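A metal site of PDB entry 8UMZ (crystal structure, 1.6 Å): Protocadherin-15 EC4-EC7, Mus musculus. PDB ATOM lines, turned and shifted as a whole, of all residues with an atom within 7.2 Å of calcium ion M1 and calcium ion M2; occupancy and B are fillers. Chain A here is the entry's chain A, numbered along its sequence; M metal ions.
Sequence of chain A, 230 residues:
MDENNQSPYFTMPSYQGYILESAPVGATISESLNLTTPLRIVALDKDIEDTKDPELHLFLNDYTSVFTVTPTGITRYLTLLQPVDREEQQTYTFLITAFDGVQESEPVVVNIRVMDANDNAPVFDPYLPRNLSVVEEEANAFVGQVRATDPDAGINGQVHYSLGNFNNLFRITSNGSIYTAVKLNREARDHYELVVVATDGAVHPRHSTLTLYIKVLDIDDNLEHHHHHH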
ATOM      1  N   GLU A  21      -0.643 -19.072 -13.943  1.00  0.00           N
ATOM      2  CA  GLU A  21       0.096 -18.121 -13.130  1.00  0.00           C
ATOM      3  C   GLU A  21       1.197 -17.417 -13.951  1.00  0.00           C
ATOM      4  O   GLU A  21       1.626 -16.327 -13.612  1.00  0.00           O
ATOM      5  CB  GLU A  21       0.769 -18.742 -11.898  1.00  0.00           C
ATOM      6  CG  GLU A  21       1.795 -19.856 -12.182  1.00  0.00           C
ATOM      7  CD  GLU A  21       2.281 -20.441 -10.876  1.00  0.00           C
ATOM      8  OE1 GLU A  21       2.468 -19.697  -9.965  1.00  0.00           O
ATOM      9  OE2 GLU A  21       2.574 -21.706 -10.794  1.00  0.00           O
ATOM     10  N   ASP A  85       0.551 -15.717  -8.494  1.00  0.00           N
ATOM     11  CA  ASP A  85       1.459 -16.779  -8.089  1.00  0.00           C
ATOM     12  C   ASP A  85       0.663 -17.848  -7.379  1.00  0.00           C
ATOM     13  O   ASP A  85       0.161 -17.618  -6.291  1.00  0.00           O
ATOM     14  CB  ASP A  85       2.570 -16.164  -7.232  1.00  0.00           C
ATOM     15  CG  ASP A  85       3.527 -17.203  -6.659  1.00  0.00           C
ATOM     16  OD1 ASP A  85       3.543 -18.310  -7.165  1.00  0.00           O
ATOM     17  OD2 ASP A  85       4.231 -16.890  -5.741  1.00  0.00           O
ATOM     18  N   ARG A  86       0.688 -19.086  -7.918  1.00  0.00           N
ATOM     19  CA  ARG A  86      -0.141 -20.124  -7.390  1.00  0.00           C
ATOM     20  C   ARG A  86       0.445 -20.537  -6.042  1.00  0.00           C
ATOM     21  O   ARG A  86      -0.303 -20.902  -5.155  1.00  0.00           O
ATOM     22  CB  ARG A  86      -0.265 -21.260  -8.403  1.00  0.00           C
ATOM     23  CG  ARG A  86      -1.307 -22.281  -7.976  1.00  0.00           C
ATOM     24  CD  ARG A  86      -0.908 -23.632  -8.515  1.00  0.00           C
ATOM     25  NE  ARG A  86       0.298 -24.122  -7.867  1.00  0.00           N
ATOM     26  CZ  ARG A  86       0.383 -24.596  -6.628  1.00  0.00           C
ATOM     27  NH1 ARG A  86      -0.681 -24.684  -5.850  1.00  0.00           N
ATOM     28  NH2 ARG A  86       1.555 -25.016  -6.182  1.00  0.00           N
ATOM     29  N   GLU A  87       1.771 -20.371  -5.873  1.00  0.00           N
ATOM     30  CA  GLU A  87       2.401 -20.823  -4.641  1.00  0.00           C
ATOM     31  C   GLU A  87       2.130 -19.831  -3.494  1.00  0.00           C
ATOM     32  O   GLU A  87       2.328 -20.169  -2.329  1.00  0.00           O
ATOM     33  CB  GLU A  87       3.907 -20.972  -4.846  1.00  0.00           C
ATOM     34  CG  GLU A  87       4.305 -22.252  -5.574  1.00  0.00           C
ATOM     35  CD  GLU A  87       3.963 -22.342  -7.046  1.00  0.00           C
ATOM     36  OE1 GLU A  87       4.406 -21.470  -7.808  1.00  0.00           O
ATOM     37  OE2 GLU A  87       3.281 -23.339  -7.444  1.00  0.00           O
ATOM     38  N   MET A 115      -4.091 -21.529 -12.283  1.00  0.00           N
ATOM     39  CA  MET A 115      -3.570 -22.828 -12.692  1.00  0.00           C
ATOM     40  C   MET A 115      -2.061 -22.851 -12.504  1.00  0.00           C
ATOM     41  O   MET A 115      -1.389 -21.827 -12.581  1.00  0.00           O
ATOM     42  CB  MET A 115      -3.911 -23.185 -14.136  1.00  0.00           C
ATOM     43  CG  MET A 115      -5.390 -23.132 -14.493  1.00  0.00           C
ATOM     44  SD  MET A 115      -6.411 -24.225 -13.490  1.00  0.00           S
ATOM     45  CE  MET A 115      -5.964 -25.814 -14.203  1.00  0.00           C
ATOM     46  N   ASP A 116      -1.525 -24.038 -12.210  1.00  0.00           N
ATOM     47  CA  ASP A 116      -0.107 -24.158 -11.944  1.00  0.00           C
ATOM     48  C   ASP A 116       0.685 -24.236 -13.230  1.00  0.00           C
ATOM     49  O   ASP A 116       0.388 -24.972 -14.180  1.00  0.00           O
ATOM     50  CB  ASP A 116       0.117 -25.400 -11.085  1.00  0.00           C
ATOM     51  CG  ASP A 116       1.550 -25.522 -10.616  1.00  0.00           C
ATOM     52  OD1 ASP A 116       2.057 -24.570 -10.052  1.00  0.00           O
ATOM     53  OD2 ASP A 116       2.122 -26.651 -10.792  1.00  0.00           O
ATOM     54  N   ALA A 117       1.770 -23.475 -13.241  1.00  0.00           N
ATOM     55  CA  ALA A 117       2.812 -23.609 -14.222  1.00  0.00           C
ATOM     56  C   ALA A 117       3.947 -24.367 -13.519  1.00  0.00           C
ATOM     57  O   ALA A 117       4.122 -24.245 -12.312  1.00  0.00           O
ATOM     58  CB  ALA A 117       3.293 -22.244 -14.652  1.00  0.00           C
ATOM     59  N   ASN A 118       4.719 -25.130 -14.289  1.00  0.00           N
ATOM     60  CA  ASN A 118       5.962 -25.664 -13.755  1.00  0.00           C
ATOM     61  C   ASN A 118       7.057 -24.608 -13.772  1.00  0.00           C
ATOM     62  O   ASN A 118       7.991 -24.718 -14.579  1.00  0.00           O
ATOM     63  CB  ASN A 118       6.404 -26.922 -14.498  1.00  0.00           C
ATOM     64  CG  ASN A 118       7.525 -27.537 -13.718  1.00  0.00           C
ATOM     65  OD1 ASN A 118       7.506 -27.476 -12.494  1.00  0.00           O
ATOM     66  ND2 ASN A 118       8.548 -27.994 -14.434  1.00  0.00           N
ATOM     67  N   ASP A 119       6.960 -23.633 -12.860  1.00  0.00           N
ATOM     68  CA  ASP A 119       7.761 -22.406 -12.827  1.00  0.00           C
ATOM     69  C   ASP A 119       8.860 -22.454 -11.763  1.00  0.00           C
ATOM     70  O   ASP A 119       9.601 -21.486 -11.524  1.00  0.00           O
ATOM     71  CB  ASP A 119       6.872 -21.146 -12.743  1.00  0.00           C
ATOM     72  CG  ASP A 119       5.967 -20.992 -11.528  1.00  0.00           C
ATOM     73  OD1 ASP A 119       5.701 -22.011 -10.870  1.00  0.00           O
ATOM     74  OD2 ASP A 119       5.560 -19.806 -11.168  1.00  0.00           O
ATOM     75  N   ASN A 120       9.009 -23.622 -11.124  1.00  0.00           N
ATOM     76  CA  ASN A 120      10.000 -23.794 -10.079  1.00  0.00           C
ATOM     77  C   ASN A 120      10.811 -25.049 -10.409  1.00  0.00           C
ATOM     78  O   ASN A 120      10.249 -26.061 -10.829  1.00  0.00           O
ATOM     79  CB  ASN A 120       9.435 -23.855  -8.660  1.00  0.00           C
ATOM     80  CG  ASN A 120       8.802 -22.542  -8.253  1.00  0.00           C
ATOM     81  OD1 ASN A 120       7.616 -22.341  -8.467  1.00  0.00           O
ATOM     82  ND2 ASN A 120       9.566 -21.721  -7.567  1.00  0.00           N
ATOM     83  N   ALA A 121      12.120 -24.947 -10.218  1.00  0.00           N
ATOM     84  CA  ALA A 121      12.972 -26.116 -10.188  1.00  0.00           C
ATOM     85  C   ALA A 121      13.035 -26.652  -8.762  1.00  0.00           C
ATOM     86  O   ALA A 121      12.857 -25.923  -7.804  1.00  0.00           O
ATOM     87  CB  ALA A 121      14.350 -25.765 -10.721  1.00  0.00           C
ATOM     88  N   PRO A 122      13.394 -27.943  -8.545  1.00  0.00           N
ATOM     89  CA  PRO A 122      13.666 -28.419  -7.200  1.00  0.00           C
ATOM     90  C   PRO A 122      14.781 -27.573  -6.574  1.00  0.00           C
ATOM     91  O   PRO A 122      15.730 -27.159  -7.241  1.00  0.00           O
ATOM     92  CB  PRO A 122      14.118 -29.875  -7.470  1.00  0.00           C
ATOM     93  CG  PRO A 122      13.387 -30.265  -8.693  1.00  0.00           C
ATOM     94  CD  PRO A 122      13.480 -29.025  -9.548  1.00  0.00           C
ATOM     95  N   ASP A 150      10.207 -29.061  -4.165  1.00  0.00           N
ATOM     96  CA  ASP A 150       9.731 -28.281  -5.290  1.00  0.00           C
ATOM     97  C   ASP A 150       8.333 -27.838  -4.924  1.00  0.00           C
ATOM     98  O   ASP A 150       7.459 -28.684  -4.696  1.00  0.00           O
ATOM     99  CB  ASP A 150       9.719 -29.177  -6.527  1.00  0.00           C
ATOM    100  CG  ASP A 150       9.422 -28.497  -7.854  1.00  0.00           C
ATOM    101  OD1 ASP A 150       8.467 -27.664  -7.920  1.00  0.00           O
ATOM    102  OD2 ASP A 150      10.121 -28.787  -8.807  1.00  0.00           O
ATOM    103  N   PRO A 151       8.075 -26.513  -4.893  1.00  0.00           N
ATOM    104  CA  PRO A 151       6.803 -25.999  -4.372  1.00  0.00           C
ATOM    105  C   PRO A 151       5.653 -26.105  -5.390  1.00  0.00           C
ATOM    106  O   PRO A 151       4.504 -25.765  -4.999  1.00  0.00           O
ATOM    107  CB  PRO A 151       7.193 -24.547  -4.007  1.00  0.00           C
ATOM    108  CG  PRO A 151       8.173 -24.169  -5.091  1.00  0.00           C
ATOM    109  CD  PRO A 151       8.946 -25.450  -5.399  1.00  0.00           C
ATOM    110  N   ASP A 152       5.906 -26.504  -6.666  1.00  0.00           N
ATOM    111  CA  ASP A 152       4.837 -26.607  -7.654  1.00  0.00           C
ATOM    112  C   ASP A 152       3.874 -27.740  -7.319  1.00  0.00           C
ATOM    113  O   ASP A 152       4.103 -28.490  -6.377  1.00  0.00           O
ATOM    114  CB  ASP A 152       5.323 -26.747  -9.093  1.00  0.00           C
ATOM    115  CG  ASP A 152       6.257 -25.651  -9.548  1.00  0.00           C
ATOM    116  OD1 ASP A 152       5.859 -24.503  -9.458  1.00  0.00           O
ATOM    117  OD2 ASP A 152       7.284 -25.977 -10.167  1.00  0.00           O
ATOM    118  N   ALA A 153       2.783 -27.831  -8.089  1.00  0.00           N
ATOM    119  CA  ALA A 153       1.683 -28.731  -7.807  1.00  0.00           C
ATOM    120  C   ALA A 153       1.825 -30.049  -8.549  1.00  0.00           C
ATOM    121  O   ALA A 153       2.201 -30.118  -9.719  1.00  0.00           O
ATOM    122  CB  ALA A 153       0.377 -28.080  -8.232  1.00  0.00           C
ATOM    123  N   ILE A 155       2.601 -33.286 -10.223  1.00  0.00           N
ATOM    124  CA  ILE A 155       3.817 -33.882 -10.819  1.00  0.00           C
ATOM    125  C   ILE A 155       4.873 -32.795 -10.964  1.00  0.00           C
ATOM    126  O   ILE A 155       6.089 -33.035 -10.870  1.00  0.00           O
ATOM    127  CB  ILE A 155       3.571 -34.532 -12.174  1.00  0.00           C
ATOM    128  CG1 ILE A 155       3.053 -33.501 -13.218  1.00  0.00           C
ATOM    129  CG2 ILE A 155       2.711 -35.753 -12.097  1.00  0.00           C
ATOM    130  CD1 ILE A 155       2.624 -34.158 -14.516  1.00  0.00           C
ATOM    131  N   ASN A 156       4.426 -31.532 -11.080  1.00  0.00           N
ATOM    132  CA  ASN A 156       5.365 -30.434 -11.240  1.00  0.00           C
ATOM    133  C   ASN A 156       6.194 -30.217  -9.962  1.00  0.00           C
ATOM    134  O   ASN A 156       7.206 -29.552 -10.057  1.00  0.00           O
ATOM    135  CB  ASN A 156       4.650 -29.139 -11.689  1.00  0.00           C
ATOM    136  CG  ASN A 156       3.879 -29.238 -12.979  1.00  0.00           C
ATOM    137  OD1 ASN A 156       4.171 -30.069 -13.855  1.00  0.00           O
ATOM    138  ND2 ASN A 156       2.865 -28.365 -13.133  1.00  0.00           N
ATOM    139  N   GLY A 157       5.744 -30.735  -8.804  1.00  0.00           N
ATOM    140  CA  GLY A 157       6.407 -30.600  -7.521  1.00  0.00           C
ATOM    141  C   GLY A 157       6.980 -31.930  -7.013  1.00  0.00           C
ATOM    142  O   GLY A 157       7.565 -31.915  -5.949  1.00  0.00           O
ATOM    143  N   GLN A 158       6.878 -33.017  -7.795  1.00  0.00           N
ATOM    144  CA  GLN A 158       7.456 -34.307  -7.392  1.00  0.00           C
ATOM    145  C   GLN A 158       8.880 -34.441  -7.896  1.00  0.00           C
ATOM    146  O   GLN A 158       9.206 -34.101  -9.030  1.00  0.00           O
ATOM    147  CB  GLN A 158       6.582 -35.465  -7.824  1.00  0.00           C
ATOM    148  CG  GLN A 158       5.277 -35.511  -7.056  1.00  0.00           C
ATOM    149  CD  GLN A 158       4.319 -36.459  -7.737  1.00  0.00           C
ATOM    150  OE1 GLN A 158       4.663 -37.324  -8.562  1.00  0.00           O
ATOM    151  NE2 GLN A 158       3.051 -36.245  -7.465  1.00  0.00           N
ATOM    152  N   THR A 199      15.181 -33.681 -10.408  1.00  0.00           N
ATOM    153  CA  THR A 199      14.333 -33.382 -11.580  1.00  0.00           C
ATOM    154  C   THR A 199      12.875 -33.539 -11.153  1.00  0.00           C
ATOM    155  O   THR A 199      12.502 -34.468 -10.452  1.00  0.00           O
ATOM    156  CB  THR A 199      14.619 -34.342 -12.722  1.00  0.00           C
ATOM    157  OG1 THR A 199      16.020 -34.307 -13.077  1.00  0.00           O
ATOM    158  CG2 THR A 199      13.785 -34.073 -13.959  1.00  0.00           C
ATOM    159  N   ASP A 200      12.019 -32.569 -11.497  1.00  0.00           N
ATOM    160  CA  ASP A 200      10.602 -32.764 -11.230  1.00  0.00           C
ATOM    161  C   ASP A 200       9.933 -33.673 -12.261  1.00  0.00           C
ATOM    162  O   ASP A 200      10.531 -34.100 -13.246  1.00  0.00           O
ATOM    163  CB  ASP A 200       9.930 -31.405 -11.020  1.00  0.00           C
ATOM    164  CG  ASP A 200       9.988 -30.438 -12.192  1.00  0.00           C
ATOM    165  OD1 ASP A 200       9.960 -30.931 -13.289  1.00  0.00           O
ATOM    166  OD2 ASP A 200      10.010 -29.146 -11.933  1.00  0.00           O
ATOM    167  N   GLY A 201       8.643 -33.973 -11.989  1.00  0.00           N
ATOM    168  CA  GLY A 201       7.815 -34.842 -12.798  1.00  0.00           C
ATOM    169  C   GLY A 201       7.021 -34.140 -13.901  1.00  0.00           C
ATOM    170  O   GLY A 201       6.213 -34.795 -14.528  1.00  0.00           O
ATOM    171  N   ALA A 202       7.309 -32.897 -14.245  1.00  0.00           N
ATOM    172  CA  ALA A 202       6.510 -32.179 -15.223  1.00  0.00           C
ATOM    173  C   ALA A 202       6.641 -32.764 -16.622  1.00  0.00           C
ATOM    174  O   ALA A 202       7.659 -33.365 -16.987  1.00  0.00           O
ATOM    175  CB  ALA A 202       6.921 -30.757 -15.214  1.00  0.00           C
ATOM    176  N   HIS A 204       7.158 -30.865 -19.036  1.00  0.00           N
ATOM    177  CA  HIS A 204       8.304 -30.083 -19.474  1.00  0.00           C
ATOM    178  C   HIS A 204       9.199 -29.975 -18.240  1.00  0.00           C
ATOM    179  O   HIS A 204       9.043 -29.032 -17.477  1.00  0.00           O
ATOM    180  CB  HIS A 204       7.812 -28.734 -20.020  1.00  0.00           C
ATOM    181  CG  HIS A 204       6.838 -28.836 -21.152  1.00  0.00           C
ATOM    182  ND1 HIS A 204       5.556 -28.315 -21.089  1.00  0.00           N
ATOM    183  CD2 HIS A 204       6.963 -29.372 -22.387  1.00  0.00           C
ATOM    184  CE1 HIS A 204       4.948 -28.552 -22.259  1.00  0.00           C
ATOM    185  NE2 HIS A 204       5.788 -29.156 -23.058  1.00  0.00           N
ATOM    186  N   PRO A 205      10.032 -30.992 -17.919  1.00  0.00           N
ATOM    187  CA  PRO A 205      10.665 -31.049 -16.589  1.00  0.00           C
ATOM    188  C   PRO A 205      11.624 -29.908 -16.332  1.00  0.00           C
ATOM    189  O   PRO A 205      12.214 -29.366 -17.272  1.00  0.00           O
ATOM    190  CB  PRO A 205      11.379 -32.404 -16.619  1.00  0.00           C
ATOM    191  CG  PRO A 205      11.596 -32.650 -18.088  1.00  0.00           C
ATOM    192  CD  PRO A 205      10.267 -32.217 -18.679  1.00  0.00           C
ATOM    193  N   ARG A 206      11.811 -29.570 -15.059  1.00  0.00           N
ATOM    194  CA  ARG A 206      12.885 -28.661 -14.632  1.00  0.00           C
ATOM    195  C   ARG A 206      13.796 -29.456 -13.694  1.00  0.00           C
ATOM    196  O   ARG A 206      13.334 -30.412 -13.061  1.00  0.00           O
ATOM    197  CB  ARG A 206      12.379 -27.398 -13.962  1.00  0.00           C
ATOM    198  CG  ARG A 206      11.727 -26.390 -14.900  1.00  0.00           C
ATOM    199  CD  ARG A 206      11.367 -25.145 -14.125  1.00  0.00           C
ATOM    200  NE  ARG A 206      10.783 -24.067 -14.944  1.00  0.00           N
ATOM    201  CZ  ARG A 206      11.513 -23.216 -15.683  1.00  0.00           C
ATOM    202  NH1 ARG A 206      12.828 -23.338 -15.738  1.00  0.00           N
ATOM    203  NH2 ARG A 206      10.929 -22.267 -16.414  1.00  0.00           N
HETATM  204 CA    CA M   1       8.684 -27.800 -10.481  1.00  0.00          CA
HETATM  205 CA    CA M   2       3.968 -23.255  -9.995  1.00  0.00          CA
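Within 4 Å of calcium ion M1: Asn 118, Asn 120, Asp 150, Asp 152, Asn 156 and Asp 200. The nearest printed residue that does not touch calcium ion M1 is Ala 121 (4.5 Å).
The side-chain carboxylate (OD2) of Asp 152 binds calcium ion M1 (2.3 Å). Calcium ion M1 is bound by O of Asn 156. Calcium ion M1 is bound by the side-chain amide oxygen (OD1) of Asn 118 (2.4 Å). Calcium ion M1 is bound by O of Asn 120 (2.4 Å). Calcium ion M1 is bound by OD2 of Asp 200, 2.4 Å away. OD2 of Asp 150 is bound to calcium ion M1, at 2.4 Å. The side-chain carboxylate (OD1) of Asp 150 binds calcium ion M1. Calcium ion M1 has seven donor atoms within binding distance.
Calcium ion M2 is bound by OE2 of Glu 21 (2.2 Å), OD1 of Asp 119 (2.3 Å), OD1 of Asp 116 (2.3 Å), OD1 of Asp 152 (2.3 Å), O of Ala 117 (2.5 Å), OE2 of Glu 87 (2.6 Å) and OE1 of Glu 87 (2.9 Å). Calcium ion M2 has seven donor atoms within binding distance.
Six residues have an atom within 4 Å of calcium ion M2: Glu 21, Glu 87, Asp 116, Ala 117, Asp 119 and Asp 152. Along chain A the residues within 4 Å of calcium ion M2 span positions 21 to 152.
OE2 of Glu 87 lies close to NH2 of Arg 86 (2.7 Å). The side-chain carboxylate (OD2) of Asp 116 is in hydrogen-bond range of the backbone NH (N) of Ala 153 (3.0 Å). The guanidinium group (NE) of Arg 86 lies close to the side-chain carboxylate (OD1) of Asp 116 (2.8 Å). OD2 of Asp 116 is in hydrogen-bond range of ND2 of Asn 156, 3.0 Å away. ND2 of Asn 118 lies within hydrogen-bond range of O of His 204 (3.3 Å). N of Glu 87 lies within hydrogen-bond range of OD1 of Asp 85 (3.0 Å). The side-chain carboxylate (OE1) of Glu 21 lies within hydrogen-bond range of the backbone NH (N) of Arg 86, at 2.8 Å. N of Glu 21 lies within hydrogen-bond range of O of Met 115, at 3.2 Å.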
